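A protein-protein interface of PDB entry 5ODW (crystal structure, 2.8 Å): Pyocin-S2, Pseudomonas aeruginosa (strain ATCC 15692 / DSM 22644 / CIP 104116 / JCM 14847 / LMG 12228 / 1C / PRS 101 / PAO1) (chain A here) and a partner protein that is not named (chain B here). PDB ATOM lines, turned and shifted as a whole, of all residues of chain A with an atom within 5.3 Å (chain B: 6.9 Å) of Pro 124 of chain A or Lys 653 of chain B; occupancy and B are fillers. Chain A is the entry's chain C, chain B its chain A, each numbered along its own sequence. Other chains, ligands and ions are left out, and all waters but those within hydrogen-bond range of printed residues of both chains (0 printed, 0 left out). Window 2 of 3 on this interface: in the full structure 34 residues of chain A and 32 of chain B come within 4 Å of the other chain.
Arg 123 of chain A touches none of the printed residues of chain B.
Pro 124 of chain A touches just one residue of chain B: Lys 653 (3.5 Å).
Of the printed residues of chain B, Asn 126 of chain A touches Lys 653 (3.9 Å) and Pro 654 (3.1 Å).
Ala 648 of chain B touches none of the printed residues of chain A.
Printed residues of chain A within 4 Å of Ser 652 of chain B: Tyr 128 (3.6 Å) and Arg 158 (2.7 Å).
Of the printed residues of chain A, Lys 653 of chain B touches Pro 124 (3.5 Å), Asn 126 (3.9 Å) and Arg 158 (3.98 Å).
Printed residues of chain A within 4 Å of Pro 654 of chain B: Asn 126 (3.1 Å) and Tyr 128 (3.6 Å).
Printed residues of chain A within 4 Å of Thr 655 of chain B: Ala 125.
The nearest residue of chain B that does not touch Pro 124 of chain A is Thr 655 of chain B (6.8 Å).
The nearest printed residue of chain A that does not touch Lys 653 of chain B is Tyr 128 of chain A (5.0 Å).
The backbone carbonyl oxygen (O) of Ser 652 of chain B is in hydrogen-bond range of the guanidinium group (NH2) of Arg 158 of chain A (2.7 Å).
The side-chain amide oxygen (OD1) of Asn 126 of chain A sits at hydrogen-bond distance from the backbone NH (N) of Thr 129 of chain A (2.8 Å).
The backbone carbonyl oxygen (O) of Leu 649 of chain B sits at hydrogen-bond distance from the side-chain hydroxyl (OG) of Ser 652 of chain B (3.1 Å).
The side-chain hydroxyl of Ser 652 of chain B lies within hydrogen-bond range of the backbone carbonyl oxygen of Ala 648 of chain B (3.1 Å).
OD1 of Asn 126 of chain A is in hydrogen-bond range of N of Tyr 128 of chain A.
Of the 8 printed residues of chain A, 5 touch a printed residue of chain B.
Along chain A the printed residues that touch a printed residue of chain B span positions 124 to 158.
Hydrophobic or aromatic side chains of chain B that line the printed part of chain A: Pro 654.
Among the printed residues, 8 pairs touch across the chains.
Among the printed residues, no Asp or Glu carboxylate lies within 4 Å of a Lys or Arg side-chain nitrogen of the other chain.
NZ of Lys 653 of chain B touches CG of Pro 124 of chain A, 3.5 Å away.
O of Ala 125 of chain A touches CG2 of Thr 655 of chain B, 3.3 Å away.
Lys 653 of chain B touches Asn 126 of chain A (C to CB, 3.9 Å).
Pro 654 of chain B touches Asn 126 of chain A (O to CB, 3.1 Å).
CE2 of Tyr 128 of chain A touches O of Ser 652 of chain B (3.6 Å).
CD of Pro 654 of chain B touches CE2 of Tyr 128 of chain A (3.6 Å).
Lys 653 of chain B touches Arg 158 of chain A.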
ATOM      1  N   ASP A 122     -18.240   9.574  32.020  1.00  0.00           N
ATOM      2  CA  ASP A 122     -18.583  10.454  30.896  1.00  0.00           C
ATOM      3  C   ASP A 122     -17.538  10.426  29.752  1.00  0.00           C
ATOM      4  O   ASP A 122     -17.341  11.431  29.056  1.00  0.00           O
ATOM      5  CB  ASP A 122     -18.900  11.895  31.356  1.00  0.00           C
ATOM      6  CG  ASP A 122     -20.353  12.119  31.753  1.00  0.00           C
ATOM      7  OD1 ASP A 122     -21.178  12.432  30.858  1.00  0.00           O
ATOM      8  OD2 ASP A 122     -20.662  12.012  32.956  1.00  0.00           O
ATOM      9  N   ARG A 123     -16.916   9.249  29.529  1.00  0.00           N
ATOM     10  CA  ARG A 123     -15.980   9.011  28.433  1.00  0.00           C
ATOM     11  C   ARG A 123     -16.802   8.417  27.301  1.00  0.00           C
ATOM     12  O   ARG A 123     -17.746   7.668  27.590  1.00  0.00           O
ATOM     13  CB  ARG A 123     -14.908   7.989  28.821  1.00  0.00           C
ATOM     14  CG  ARG A 123     -13.765   8.524  29.660  1.00  0.00           C
ATOM     15  CD  ARG A 123     -12.763   7.422  29.960  1.00  0.00           C
ATOM     16  NE  ARG A 123     -13.405   6.211  30.486  1.00  0.00           N
ATOM     17  CZ  ARG A 123     -12.823   5.017  30.543  1.00  0.00           C
ATOM     18  NH1 ARG A 123     -13.483   3.974  31.028  1.00  0.00           N
ATOM     19  NH2 ARG A 123     -11.577   4.858  30.118  1.00  0.00           N
ATOM     20  N   PRO A 124     -16.447   8.692  26.015  1.00  0.00           N
ATOM     21  CA  PRO A 124     -17.218   8.116  24.892  1.00  0.00           C
ATOM     22  C   PRO A 124     -17.281   6.593  24.918  1.00  0.00           C
ATOM     23  O   PRO A 124     -16.305   5.941  25.277  1.00  0.00           O
ATOM     24  CB  PRO A 124     -16.483   8.635  23.649  1.00  0.00           C
ATOM     25  CG  PRO A 124     -15.130   9.047  24.134  1.00  0.00           C
ATOM     26  CD  PRO A 124     -15.351   9.552  25.515  1.00  0.00           C
ATOM     27  N   ALA A 125     -18.436   6.053  24.546  1.00  0.00           N
ATOM     28  CA  ALA A 125     -18.657   4.613  24.541  1.00  0.00           C
ATOM     29  C   ALA A 125     -17.868   3.854  23.480  1.00  0.00           C
ATOM     30  O   ALA A 125     -17.798   4.246  22.319  1.00  0.00           O
ATOM     31  CB  ALA A 125     -20.141   4.300  24.422  1.00  0.00           C
ATOM     32  N   ASN A 126     -17.284   2.751  23.922  1.00  0.00           N
ATOM     33  CA  ASN A 126     -16.494   1.853  23.096  1.00  0.00           C
ATOM     34  C   ASN A 126     -16.348   0.525  23.841  1.00  0.00           C
ATOM     35  O   ASN A 126     -16.815   0.384  24.969  1.00  0.00           O
ATOM     36  CB  ASN A 126     -15.148   2.462  22.702  1.00  0.00           C
ATOM     37  CG  ASN A 126     -14.238   2.678  23.879  1.00  0.00           C
ATOM     38  OD1 ASN A 126     -14.223   1.885  24.811  1.00  0.00           O
ATOM     39  ND2 ASN A 126     -13.465   3.751  23.841  1.00  0.00           N
ATOM     40  N   TYR A 128     -13.759  -0.844  25.232  1.00  0.00           N
ATOM     41  CA  TYR A 128     -12.955  -0.657  26.430  1.00  0.00           C
ATOM     42  C   TYR A 128     -13.726  -0.093  27.630  1.00  0.00           C
ATOM     43  O   TYR A 128     -13.482  -0.488  28.765  1.00  0.00           O
ATOM     44  CB  TYR A 128     -11.777   0.263  26.132  1.00  0.00           C
ATOM     45  CG  TYR A 128     -10.723  -0.315  25.221  1.00  0.00           C
ATOM     46  CD1 TYR A 128      -9.981  -1.423  25.599  1.00  0.00           C
ATOM     47  CD2 TYR A 128     -10.446   0.270  23.997  1.00  0.00           C
ATOM     48  CE1 TYR A 128      -9.005  -1.941  24.773  1.00  0.00           C
ATOM     49  CE2 TYR A 128      -9.473  -0.243  23.167  1.00  0.00           C
ATOM     50  CZ  TYR A 128      -8.756  -1.346  23.562  1.00  0.00           C
ATOM     51  OH  TYR A 128      -7.789  -1.853  22.734  1.00  0.00           O
ATOM     52  N   THR A 129     -14.633   0.845  27.383  1.00  0.00           N
ATOM     53  CA  THR A 129     -15.393   1.487  28.458  1.00  0.00           C
ATOM     54  C   THR A 129     -16.631   0.737  28.938  1.00  0.00           C
ATOM     55  O   THR A 129     -17.276   1.157  29.891  1.00  0.00           O
ATOM     56  CB  THR A 129     -15.821   2.921  28.091  1.00  0.00           C
ATOM     57  OG1 THR A 129     -16.936   2.877  27.197  1.00  0.00           O
ATOM     58  CG2 THR A 129     -14.681   3.679  27.444  1.00  0.00           C
ATOM     59  N   ARG A 158      -2.975  -0.884  26.830  1.00  0.00           N
ATOM     60  CA  ARG A 158      -4.335  -0.355  26.713  1.00  0.00           C
ATOM     61  C   ARG A 158      -5.324  -1.124  27.590  1.00  0.00           C
ATOM     62  O   ARG A 158      -6.076  -0.490  28.320  1.00  0.00           O
ATOM     63  CB  ARG A 158      -4.796  -0.279  25.242  1.00  0.00           C
ATOM     64  CG  ARG A 158      -6.110   0.488  25.054  1.00  0.00           C
ATOM     65  CD  ARG A 158      -5.954   1.868  24.427  1.00  0.00           C
ATOM     66  NE  ARG A 158      -7.219   2.325  23.831  1.00  0.00           N
ATOM     67  CZ  ARG A 158      -8.016   3.248  24.360  1.00  0.00           C
ATOM     68  NH1 ARG A 158      -7.673   3.864  25.486  1.00  0.00           N
ATOM     69  NH2 ARG A 158      -9.155   3.576  23.760  1.00  0.00           N
ATOM     70  N   ALA B 648      -7.013   2.487  12.103  1.00  0.00           N
ATOM     71  CA  ALA B 648      -6.502   2.999  13.366  1.00  0.00           C
ATOM     72  C   ALA B 648      -7.534   3.728  14.209  1.00  0.00           C
ATOM     73  O   ALA B 648      -7.576   3.584  15.424  1.00  0.00           O
ATOM     74  CB  ALA B 648      -5.307   3.899  13.107  1.00  0.00           C
ATOM     75  N   LEU B 649      -8.366   4.517  13.548  1.00  0.00           N
ATOM     76  CA  LEU B 649      -9.400   5.314  14.213  1.00  0.00           C
ATOM     77  C   LEU B 649     -10.431   4.442  14.922  1.00  0.00           C
ATOM     78  O   LEU B 649     -10.774   4.699  16.068  1.00  0.00           O
ATOM     79  CB  LEU B 649     -10.093   6.232  13.204  1.00  0.00           C
ATOM     80  CG  LEU B 649      -9.408   7.573  12.929  1.00  0.00           C
ATOM     81  CD1 LEU B 649      -8.063   7.382  12.242  1.00  0.00           C
ATOM     82  CD2 LEU B 649     -10.314   8.486  12.114  1.00  0.00           C
ATOM     83  N   TYR B 650     -10.907   3.405  14.245  1.00  0.00           N
ATOM     84  CA  TYR B 650     -11.813   2.429  14.843  1.00  0.00           C
ATOM     85  C   TYR B 650     -11.114   1.591  15.893  1.00  0.00           C
ATOM     86  O   TYR B 650     -11.623   1.478  16.995  1.00  0.00           O
ATOM     87  CB  TYR B 650     -12.468   1.504  13.800  1.00  0.00           C
ATOM     88  CG  TYR B 650     -13.361   0.455  14.436  1.00  0.00           C
ATOM     89  CD1 TYR B 650     -14.681   0.742  14.771  1.00  0.00           C
ATOM     90  CD2 TYR B 650     -12.873  -0.816  14.741  1.00  0.00           C
ATOM     91  CE1 TYR B 650     -15.499  -0.210  15.384  1.00  0.00           C
ATOM     92  CE2 TYR B 650     -13.681  -1.776  15.361  1.00  0.00           C
ATOM     93  CZ  TYR B 650     -14.991  -1.463  15.683  1.00  0.00           C
ATOM     94  OH  TYR B 650     -15.786  -2.386  16.302  1.00  0.00           O
ATOM     95  N   ASN B 651      -9.968   0.986  15.546  1.00  0.00           N
ATOM     96  CA  ASN B 651      -9.196   0.095  16.418  1.00  0.00           C
ATOM     97  C   ASN B 651      -8.726   0.701  17.732  1.00  0.00           C
ATOM     98  O   ASN B 651      -8.529  -0.045  18.697  1.00  0.00           O
ATOM     99  CB  ASN B 651      -8.026  -0.496  15.662  1.00  0.00           C
ATOM    100  CG  ASN B 651      -8.455  -1.460  14.595  1.00  0.00           C
ATOM    101  OD1 ASN B 651      -9.620  -1.863  14.481  1.00  0.00           O
ATOM    102  ND2 ASN B 651      -7.514  -1.864  13.794  1.00  0.00           N
ATOM    103  N   SER B 652      -8.540   2.030  17.778  1.00  0.00           N
ATOM    104  CA  SER B 652      -8.116   2.702  19.001  1.00  0.00           C
ATOM    105  C   SER B 652      -9.292   2.813  19.965  1.00  0.00           C
ATOM    106  O   SER B 652      -9.093   2.679  21.172  1.00  0.00           O
ATOM    107  CB  SER B 652      -7.510   4.072  18.699  1.00  0.00           C
ATOM    108  OG  SER B 652      -8.435   4.944  18.068  1.00  0.00           O
ATOM    109  N   LYS B 653     -10.519   3.026  19.425  1.00  0.00           N
ATOM    110  CA  LYS B 653     -11.770   3.155  20.185  1.00  0.00           C
ATOM    111  C   LYS B 653     -12.842   2.240  19.546  1.00  0.00           C
ATOM    112  O   LYS B 653     -13.772   2.757  18.909  1.00  0.00           O
ATOM    113  CB  LYS B 653     -12.223   4.626  20.222  1.00  0.00           C
ATOM    114  CG  LYS B 653     -11.290   5.531  21.022  1.00  0.00           C
ATOM    115  CD  LYS B 653     -11.560   7.008  20.789  1.00  0.00           C
ATOM    116  CE  LYS B 653     -12.611   7.537  21.743  1.00  0.00           C
ATOM    117  NZ  LYS B 653     -13.550   8.482  21.080  1.00  0.00           N
ATOM    118  N   PRO B 654     -12.695   0.883  19.635  1.00  0.00           N
ATOM    119  CA  PRO B 654     -13.688  -0.006  18.988  1.00  0.00           C
ATOM    120  C   PRO B 654     -15.085   0.103  19.584  1.00  0.00           C
ATOM    121  O   PRO B 654     -15.216   0.050  20.796  1.00  0.00           O
ATOM    122  CB  PRO B 654     -13.084  -1.411  19.154  1.00  0.00           C
ATOM    123  CG  PRO B 654     -12.154  -1.305  20.297  1.00  0.00           C
ATOM    124  CD  PRO B 654     -11.630   0.100  20.302  1.00  0.00           C
ATOM    125  N   THR B 655     -16.122   0.253  18.746  1.00  0.00           N
ATOM    126  CA  THR B 655     -17.495   0.414  19.244  1.00  0.00           C
ATOM    127  C   THR B 655     -18.380  -0.815  19.049  1.00  0.00           C
ATOM    128  O   THR B 655     -19.300  -1.017  19.849  1.00  0.00           O
ATOM    129  CB  THR B 655     -18.161   1.663  18.658  1.00  0.00           C
ATOM    130  OG1 THR B 655     -17.992   1.661  17.243  1.00  0.00           O
ATOM    131  CG2 THR B 655     -17.606   2.944  19.239  1.00  0.00           C
ATOM    132  N   ASN B 656     -18.116  -1.628  18.033  1.00  0.00           N
ATOM    133  CA  ASN B 656     -18.930  -2.817  17.775  1.00  0.00           C
ATOM    134  C   ASN B 656     -18.386  -4.045  18.492  1.00  0.00           C
ATOM    135  O   ASN B 656     -17.201  -4.341  18.390  1.00  0.00           O
ATOM    136  CB  ASN B 656     -18.994  -3.084  16.270  1.00  0.00           C
ATOM    137  CG  ASN B 656     -19.875  -4.264  15.916  1.00  0.00           C
ATOM    138  OD1 ASN B 656     -19.990  -5.225  16.672  1.00  0.00           O
ATOM    139  ND2 ASN B 656     -20.496  -4.200  14.750  1.00  0.00           N
